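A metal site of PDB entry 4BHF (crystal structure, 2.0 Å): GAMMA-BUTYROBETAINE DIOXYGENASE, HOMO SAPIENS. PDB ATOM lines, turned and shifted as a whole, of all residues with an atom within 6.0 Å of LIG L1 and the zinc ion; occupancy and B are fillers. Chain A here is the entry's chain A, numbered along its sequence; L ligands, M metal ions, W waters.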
ATOM      1  N   TRP A 181       3.913 -31.805  23.356  1.00  0.00           N
ATOM      2  CA  TRP A 181       4.532 -31.520  24.655  1.00  0.00           C
ATOM      3  C   TRP A 181       4.210 -30.126  25.127  1.00  0.00           C
ATOM      4  O   TRP A 181       3.902 -29.261  24.310  1.00  0.00           O
ATOM      5  CB  TRP A 181       6.057 -31.710  24.614  1.00  0.00           C
ATOM      6  CG  TRP A 181       6.691 -31.576  23.285  1.00  0.00           C
ATOM      7  CD1 TRP A 181       6.958 -32.571  22.387  1.00  0.00           C
ATOM      8  CD2 TRP A 181       7.182 -30.362  22.688  1.00  0.00           C
ATOM      9  NE1 TRP A 181       7.542 -32.054  21.277  1.00  0.00           N
ATOM     10  CE2 TRP A 181       7.682 -30.697  21.423  1.00  0.00           C
ATOM     11  CE3 TRP A 181       7.259 -29.029  23.110  1.00  0.00           C
ATOM     12  CZ2 TRP A 181       8.247 -29.756  20.580  1.00  0.00           C
ATOM     13  CZ3 TRP A 181       7.814 -28.103  22.270  1.00  0.00           C
ATOM     14  CH2 TRP A 181       8.302 -28.464  21.012  1.00  0.00           C
ATOM     15  N   VAL A 183       5.241 -26.656  26.924  1.00  0.00           N
ATOM     16  CA  VAL A 183       6.286 -25.733  27.345  1.00  0.00           C
ATOM     17  C   VAL A 183       5.674 -24.837  28.420  1.00  0.00           C
ATOM     18  O   VAL A 183       4.883 -23.937  28.126  1.00  0.00           O
ATOM     19  CB  VAL A 183       6.811 -24.875  26.194  1.00  0.00           C
ATOM     20  CG1 VAL A 183       7.973 -24.026  26.655  1.00  0.00           C
ATOM     21  CG2 VAL A 183       7.203 -25.747  25.011  1.00  0.00           C
ATOM     22  N   ASN A 191      14.281 -30.345  31.459  1.00  0.00           N
ATOM     23  CA  ASN A 191      14.762 -29.602  30.308  1.00  0.00           C
ATOM     24  C   ASN A 191      14.675 -28.104  30.580  1.00  0.00           C
ATOM     25  O   ASN A 191      13.664 -27.636  31.106  1.00  0.00           O
ATOM     26  CB  ASN A 191      13.881 -29.922  29.098  1.00  0.00           C
ATOM     27  CG  ASN A 191      14.551 -29.584  27.777  1.00  0.00           C
ATOM     28  OD1 ASN A 191      14.619 -28.409  27.378  1.00  0.00           O
ATOM     29  ND2 ASN A 191      15.046 -30.612  27.098  1.00  0.00           N
ATOM     30  N   ALA A 193      13.957 -25.812  28.698  1.00  0.00           N
ATOM     31  CA  ALA A 193      12.747 -25.281  28.064  1.00  0.00           C
ATOM     32  C   ALA A 193      11.592 -25.194  29.069  1.00  0.00           C
ATOM     33  O   ALA A 193      10.789 -24.286  29.013  1.00  0.00           O
ATOM     34  CB  ALA A 193      12.360 -26.144  26.878  1.00  0.00           C
ATOM     35  N   TYR A 194      11.557 -26.126  30.013  1.00  0.00           N
ATOM     36  CA  TYR A 194      10.436 -26.220  30.968  1.00  0.00           C
ATOM     37  C   TYR A 194      10.710 -25.431  32.281  1.00  0.00           C
ATOM     38  O   TYR A 194      10.418 -25.880  33.382  1.00  0.00           O
ATOM     39  CB  TYR A 194      10.150 -27.696  31.236  1.00  0.00           C
ATOM     40  CG  TYR A 194       9.744 -28.525  29.977  1.00  0.00           C
ATOM     41  CD1 TYR A 194       9.140 -27.940  28.842  1.00  0.00           C
ATOM     42  CD2 TYR A 194       9.923 -29.908  29.975  1.00  0.00           C
ATOM     43  CE1 TYR A 194       8.775 -28.716  27.744  1.00  0.00           C
ATOM     44  CE2 TYR A 194       9.557 -30.686  28.899  1.00  0.00           C
ATOM     45  CZ  TYR A 194       8.993 -30.090  27.784  1.00  0.00           C
ATOM     46  OH  TYR A 194       8.636 -30.903  26.746  1.00  0.00           O
ATOM     47  N   LEU A 199      15.910 -18.561  26.796  1.00  0.00           N
ATOM     48  CA  LEU A 199      16.549 -19.507  25.878  1.00  0.00           C
ATOM     49  C   LEU A 199      17.231 -18.692  24.811  1.00  0.00           C
ATOM     50  O   LEU A 199      16.599 -17.924  24.090  1.00  0.00           O
ATOM     51  CB  LEU A 199      15.504 -20.458  25.253  1.00  0.00           C
ATOM     52  CG  LEU A 199      14.691 -21.304  26.241  1.00  0.00           C
ATOM     53  CD1 LEU A 199      13.611 -22.124  25.554  1.00  0.00           C
ATOM     54  CD2 LEU A 199      15.598 -22.211  27.025  1.00  0.00           C
ATOM     55  N   HIS A 202      18.890 -21.398  19.535  1.00  0.00           N
ATOM     56  CA  HIS A 202      19.149 -22.816  19.433  1.00  0.00           C
ATOM     57  C   HIS A 202      18.248 -23.439  18.356  1.00  0.00           C
ATOM     58  O   HIS A 202      17.228 -22.844  17.976  1.00  0.00           O
ATOM     59  CB  HIS A 202      18.878 -23.504  20.775  1.00  0.00           C
ATOM     60  CG  HIS A 202      17.444 -23.489  21.215  1.00  0.00           C
ATOM     61  ND1 HIS A 202      16.854 -22.370  21.748  1.00  0.00           N
ATOM     62  CD2 HIS A 202      16.495 -24.457  21.213  1.00  0.00           C
ATOM     63  CE1 HIS A 202      15.593 -22.645  22.063  1.00  0.00           C
ATOM     64  NE2 HIS A 202      15.357 -23.907  21.762  1.00  0.00           N
ATOM     65  N   THR A 203      18.677 -24.593  17.868  1.00  0.00           N
ATOM     66  CA  THR A 203      17.793 -25.559  17.203  1.00  0.00           C
ATOM     67  C   THR A 203      17.373 -26.609  18.240  1.00  0.00           C
ATOM     68  O   THR A 203      18.110 -26.837  19.185  1.00  0.00           O
ATOM     69  CB  THR A 203      18.481 -26.256  16.027  1.00  0.00           C
ATOM     70  OG1 THR A 203      19.688 -26.922  16.439  1.00  0.00           O
ATOM     71  CG2 THR A 203      18.870 -25.238  14.946  1.00  0.00           C
ATOM     72  N   ASP A 204      16.196 -27.201  18.051  1.00  0.00           N
ATOM     73  CA  ASP A 204      15.707 -28.294  18.873  1.00  0.00           C
ATOM     74  C   ASP A 204      16.290 -29.623  18.494  1.00  0.00           C
ATOM     75  O   ASP A 204      16.479 -29.977  17.314  1.00  0.00           O
ATOM     76  CB  ASP A 204      14.164 -28.378  18.806  1.00  0.00           C
ATOM     77  CG  ASP A 204      13.482 -27.517  19.847  1.00  0.00           C
ATOM     78  OD1 ASP A 204      14.042 -26.446  20.159  1.00  0.00           O
ATOM     79  OD2 ASP A 204      12.396 -27.920  20.347  1.00  0.00           O
ATOM     80  N   GLN A 215       9.155 -27.672  13.272  1.00  0.00           N
ATOM     81  CA  GLN A 215       8.659 -27.526  14.598  1.00  0.00           C
ATOM     82  C   GLN A 215       7.373 -26.702  14.585  1.00  0.00           C
ATOM     83  O   GLN A 215       7.236 -25.779  13.818  1.00  0.00           O
ATOM     84  CB  GLN A 215       9.703 -26.842  15.471  1.00  0.00           C
ATOM     85  CG  GLN A 215       9.231 -26.547  16.877  1.00  0.00           C
ATOM     86  CD  GLN A 215      10.355 -26.188  17.859  1.00  0.00           C
ATOM     87  OE1 GLN A 215      10.084 -25.633  18.924  1.00  0.00           O
ATOM     88  NE2 GLN A 215      11.599 -26.496  17.506  1.00  0.00           N
ATOM     89  N   LEU A 217       4.713 -24.654  17.262  1.00  0.00           N
ATOM     90  CA  LEU A 217       4.559 -24.104  18.620  1.00  0.00           C
ATOM     91  C   LEU A 217       3.284 -23.257  18.666  1.00  0.00           C
ATOM     92  O   LEU A 217       3.118 -22.294  17.912  1.00  0.00           O
ATOM     93  CB  LEU A 217       5.763 -23.225  19.030  1.00  0.00           C
ATOM     94  CG  LEU A 217       7.094 -23.754  19.597  1.00  0.00           C
ATOM     95  CD1 LEU A 217       8.017 -22.573  19.926  1.00  0.00           C
ATOM     96  CD2 LEU A 217       6.851 -24.530  20.851  1.00  0.00           C
ATOM     97  N   GLY A 227       8.933 -13.399  27.891  1.00  0.00           N
ATOM     98  CA  GLY A 227       8.555 -14.545  27.037  1.00  0.00           C
ATOM     99  C   GLY A 227       8.316 -14.213  25.572  1.00  0.00           C
ATOM    100  O   GLY A 227       7.727 -14.999  24.848  1.00  0.00           O
ATOM    101  N   ASP A 228       8.804 -13.065  25.122  1.00  0.00           N
ATOM    102  CA  ASP A 228       8.884 -12.758  23.684  1.00  0.00           C
ATOM    103  C   ASP A 228       9.678 -13.822  22.956  1.00  0.00           C
ATOM    104  O   ASP A 228      10.596 -14.411  23.524  1.00  0.00           O
ATOM    105  CB  ASP A 228       9.576 -11.412  23.440  1.00  0.00           C
ATOM    106  CG  ASP A 228       8.904 -10.274  24.216  1.00  0.00           C
ATOM    107  OD1 ASP A 228       9.107 -10.196  25.449  1.00  0.00           O
ATOM    108  OD2 ASP A 228       8.141  -9.520  23.601  1.00  0.00           O
ATOM    109  N   SER A 229       9.341 -14.037  21.684  1.00  0.00           N
ATOM    110  CA  SER A 229      10.060 -14.950  20.823  1.00  0.00           C
ATOM    111  C   SER A 229      11.108 -14.249  19.988  1.00  0.00           C
ATOM    112  O   SER A 229      10.955 -13.076  19.641  1.00  0.00           O
ATOM    113  CB  SER A 229       9.066 -15.640  19.901  1.00  0.00           C
ATOM    114  OG  SER A 229       8.091 -16.263  20.680  1.00  0.00           O
ATOM    115  N   ASN A 292      22.203 -26.524  20.215  1.00  0.00           N
ATOM    116  CA  ASN A 292      21.516 -26.125  21.420  1.00  0.00           C
ATOM    117  C   ASN A 292      22.579 -26.082  22.561  1.00  0.00           C
ATOM    118  O   ASN A 292      23.258 -27.071  22.833  1.00  0.00           O
ATOM    119  CB  ASN A 292      20.374 -27.084  21.700  1.00  0.00           C
ATOM    120  CG  ASN A 292      19.557 -26.672  22.909  1.00  0.00           C
ATOM    121  OD1 ASN A 292      20.016 -25.845  23.725  1.00  0.00           O
ATOM    122  ND2 ASN A 292      18.389 -27.214  23.043  1.00  0.00           N
ATOM    123  N   MET A 332       4.174 -14.030  20.866  1.00  0.00           N
ATOM    124  CA  MET A 332       3.041 -14.874  20.549  1.00  0.00           C
ATOM    125  C   MET A 332       1.864 -14.533  21.485  1.00  0.00           C
ATOM    126  O   MET A 332       2.073 -14.269  22.643  1.00  0.00           O
ATOM    127  CB  MET A 332       3.416 -16.336  20.727  1.00  0.00           C
ATOM    128  CG  MET A 332       4.569 -16.804  19.830  1.00  0.00           C
ATOM    129  SD  MET A 332       4.676 -18.604  19.727  1.00  0.00           S
ATOM    130  CE  MET A 332       3.255 -18.885  18.667  1.00  0.00           C
ATOM    131  N   HIS A 347      15.919 -20.317  17.179  1.00  0.00           N
ATOM    132  CA  HIS A 347      14.895 -19.615  17.858  1.00  0.00           C
ATOM    133  C   HIS A 347      15.236 -19.552  19.343  1.00  0.00           C
ATOM    134  O   HIS A 347      16.110 -20.287  19.844  1.00  0.00           O
ATOM    135  CB  HIS A 347      13.555 -20.312  17.636  1.00  0.00           C
ATOM    136  CG  HIS A 347      13.479 -21.689  18.216  1.00  0.00           C
ATOM    137  ND1 HIS A 347      14.051 -22.784  17.604  1.00  0.00           N
ATOM    138  CD2 HIS A 347      12.877 -22.144  19.340  1.00  0.00           C
ATOM    139  CE1 HIS A 347      13.823 -23.864  18.336  1.00  0.00           C
ATOM    140  NE2 HIS A 347      13.106 -23.501  19.390  1.00  0.00           N
ATOM    141  N   GLY A 348      14.557 -18.643  20.015  1.00  0.00           N
ATOM    142  CA  GLY A 348      14.752 -18.467  21.435  1.00  0.00           C
ATOM    143  C   GLY A 348      13.608 -17.748  22.110  1.00  0.00           C
ATOM    144  O   GLY A 348      12.612 -17.408  21.494  1.00  0.00           O
ATOM    145  N   ARG A 349      13.766 -17.510  23.391  1.00  0.00           N
ATOM    146  CA  ARG A 349      12.772 -16.761  24.088  1.00  0.00           C
ATOM    147  C   ARG A 349      13.396 -16.008  25.272  1.00  0.00           C
ATOM    148  O   ARG A 349      14.420 -16.417  25.846  1.00  0.00           O
ATOM    149  CB  ARG A 349      11.632 -17.632  24.572  1.00  0.00           C
ATOM    150  CG  ARG A 349      12.016 -18.552  25.708  1.00  0.00           C
ATOM    151  CD  ARG A 349      10.901 -18.807  26.718  1.00  0.00           C
ATOM    152  NE  ARG A 349      11.541 -19.520  27.811  1.00  0.00           N
ATOM    153  CZ  ARG A 349      11.420 -20.808  28.128  1.00  0.00           C
ATOM    154  NH1 ARG A 349      10.599 -21.649  27.505  1.00  0.00           N
ATOM    155  NH2 ARG A 349      12.150 -21.249  29.154  1.00  0.00           N
ATOM    156  N   ARG A 360       2.201 -19.115  31.592  1.00  0.00           N
ATOM    157  CA  ARG A 360       2.627 -19.250  30.212  1.00  0.00           C
ATOM    158  C   ARG A 360       2.616 -20.708  29.821  1.00  0.00           C
ATOM    159  O   ARG A 360       3.126 -21.541  30.558  1.00  0.00           O
ATOM    160  CB  ARG A 360       4.018 -18.622  30.043  1.00  0.00           C
ATOM    161  CG  ARG A 360       4.444 -18.468  28.592  1.00  0.00           C
ATOM    162  CD  ARG A 360       5.851 -17.925  28.524  1.00  0.00           C
ATOM    163  NE  ARG A 360       6.291 -17.609  27.172  1.00  0.00           N
ATOM    164  CZ  ARG A 360       6.902 -18.444  26.344  1.00  0.00           C
ATOM    165  NH1 ARG A 360       7.102 -19.723  26.651  1.00  0.00           N
ATOM    166  NH2 ARG A 360       7.295 -17.992  25.155  1.00  0.00           N
ATOM    167  N   LEU A 362       2.813 -23.082  26.065  1.00  0.00           N
ATOM    168  CA  LEU A 362       2.734 -23.400  24.644  1.00  0.00           C
ATOM    169  C   LEU A 362       2.640 -24.917  24.507  1.00  0.00           C
ATOM    170  O   LEU A 362       3.202 -25.651  25.329  1.00  0.00           O
ATOM    171  CB  LEU A 362       3.946 -22.879  23.867  1.00  0.00           C
ATOM    172  CG  LEU A 362       4.613 -21.559  24.285  1.00  0.00           C
ATOM    173  CD1 LEU A 362       5.972 -21.469  23.615  1.00  0.00           C
ATOM    174  CD2 LEU A 362       3.782 -20.332  23.954  1.00  0.00           C
ATOM    175  N   TYR A 366       6.673 -31.877  16.558  1.00  0.00           N
ATOM    176  CA  TYR A 366       7.620 -31.917  15.482  1.00  0.00           C
ATOM    177  C   TYR A 366       7.046 -32.688  14.289  1.00  0.00           C
ATOM    178  O   TYR A 366       6.130 -33.495  14.444  1.00  0.00           O
ATOM    179  CB  TYR A 366       8.896 -32.624  15.941  1.00  0.00           C
ATOM    180  CG  TYR A 366       9.648 -31.958  17.088  1.00  0.00           C
ATOM    181  CD1 TYR A 366      10.128 -30.657  16.986  1.00  0.00           C
ATOM    182  CD2 TYR A 366       9.908 -32.661  18.259  1.00  0.00           C
ATOM    183  CE1 TYR A 366      10.828 -30.066  18.028  1.00  0.00           C
ATOM    184  CE2 TYR A 366      10.618 -32.093  19.298  1.00  0.00           C
ATOM    185  CZ  TYR A 366      11.077 -30.800  19.191  1.00  0.00           C
ATOM    186  OH  TYR A 366      11.787 -30.234  20.254  1.00  0.00           O
HETATM  187  C1  LIG L   1      11.604 -24.885  23.342  1.00  0.00           C
HETATM  188  C2  LIG L   1      11.469 -23.498  22.892  1.00  0.00           C
HETATM  189  C3  LIG L   1      10.229 -21.446  22.954  1.00  0.00           C
HETATM  190  C4  LIG L   1       9.434 -20.683  23.968  1.00  0.00           C
HETATM  191  O1  LIG L   1      12.518 -25.567  22.848  1.00  0.00           O
HETATM  192  O2  LIG L   1      10.774 -25.340  24.168  1.00  0.00           O
HETATM  193  O3  LIG L   1      12.269 -23.035  22.093  1.00  0.00           O
HETATM  194  O4  LIG L   1       9.060 -19.581  23.573  1.00  0.00           O
HETATM  195  N1  LIG L   1      10.435 -22.811  23.385  1.00  0.00           N
HETATM  196  O5  LIG L   1       9.222 -21.121  25.124  1.00  0.00           O
HETATM  197  N1  LG2 L   2      11.713 -29.729  24.098  1.00  0.00           N
HETATM  198  C1  LG2 L   2      10.768 -30.699  23.499  1.00  0.00           C
HETATM  199  O1  LG2 L   2      16.482 -30.137  24.243  1.00  0.00           O
HETATM  200  C2  LG2 L   2      16.318 -29.538  23.163  1.00  0.00           C
HETATM  201  O2  LG2 L   2      17.130 -29.713  22.260  1.00  0.00           O
HETATM  202  C3  LG2 L   2      15.189 -28.556  22.863  1.00  0.00           C
HETATM  203  C4  LG2 L   2      12.952 -29.652  23.242  1.00  0.00           C
HETATM  204  C5  LG2 L   2      11.021 -28.435  24.114  1.00  0.00           C
HETATM  205  C6  LG2 L   2      11.971 -30.106  25.502  1.00  0.00           C
HETATM  206  C7  LG2 L   2      13.988 -28.667  23.793  1.00  0.00           C
HETATM  207  C8  LG2 L   2      13.645 -30.977  23.007  1.00  0.00           C
HETATM  208 ZN    ZN M   1      13.416 -24.715  21.247  1.00  0.00          ZN
HETATM  209  O   HOH W   1       9.784 -18.357  21.269  1.00  0.00           O
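O5 of LIG L1 lies within salt-bridge range of NH1 of Arg 349, 2.8 Å away. ND2 of Asn 292 sits at hydrogen-bond distance from O2 of LG2 L2, at 2.9 Å. The guanidinium group of Arg 360 is in salt-bridge range of an oxygen (O4) of LIG L1 (2.9 Å). The side-chain amide nitrogen (ND2) of Asn 191 sits at hydrogen-bond distance from an oxygen (O1) of LG2 L2 (3.2 Å).
The guanidinium group (NH1) of Arg 349 is in hydrogen-bond range of the backbone carbonyl oxygen (O) of Ala 193 (3.0 Å). The backbone NH of Leu 199 lies within hydrogen-bond range of the backbone carbonyl oxygen of Arg 349, 2.8 Å away. NH2 of Arg 360 sits at hydrogen-bond distance from O of Gly 227, 3.0 Å away. The side-chain amide nitrogen (NE2) of Gln 215 lies close to the side-chain carboxylate (OD2) of Asp 204, 3.3 Å away. O of Leu 362 sits at hydrogen-bond distance from N of Val 183. OD1 of Asn 191 sits at hydrogen-bond distance from N of Ala 193.
Val 183 touches LIG L1 (CG1 to O5, 3.5 Å). Ala 193 touches LIG L1. Leu 199 touches LIG L1 (CD1 to C2, 3.7 Å). Leu 217 touches LIG L1 (CD1 to C3, 3.9 Å). Leu 362 touches LIG L1. Within 4 Å of LIG L1: Val 183, Ala 193, Leu 199, His 202, Asp 204, Leu 217, His 347, Arg 349, Arg 360 and Leu 362. The nearest printed residue that does not touch LIG L1 is Trp 181 (4.5 Å).
Three residues have an atom within 4 Å of the zinc ion: His 202, Asp 204 and His 347. Along chain A the residues within 4 Å of the zinc ion span positions 202 to 347. The nearest printed residue that does not touch the zinc ion is Gln 215 (4.2 Å).
The zinc ion is bound by an oxygen (O1) of LIG L1, the side-chain carboxylate (OD1) of Asp 204, a ring nitrogen (NE2) of His 202, an oxygen (O3) of LIG L1 and a ring nitrogen (NE2) of His 347. The zinc ion has five donor atoms within binding distance.
Water W1 lies within hydrogen-bond range of an oxygen (O4) of LIG L1 (2.7 Å), the side-chain hydroxyl of Ser 229 (2.8 Å) and the backbone carbonyl oxygen of Gly 348 (3.0 Å).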
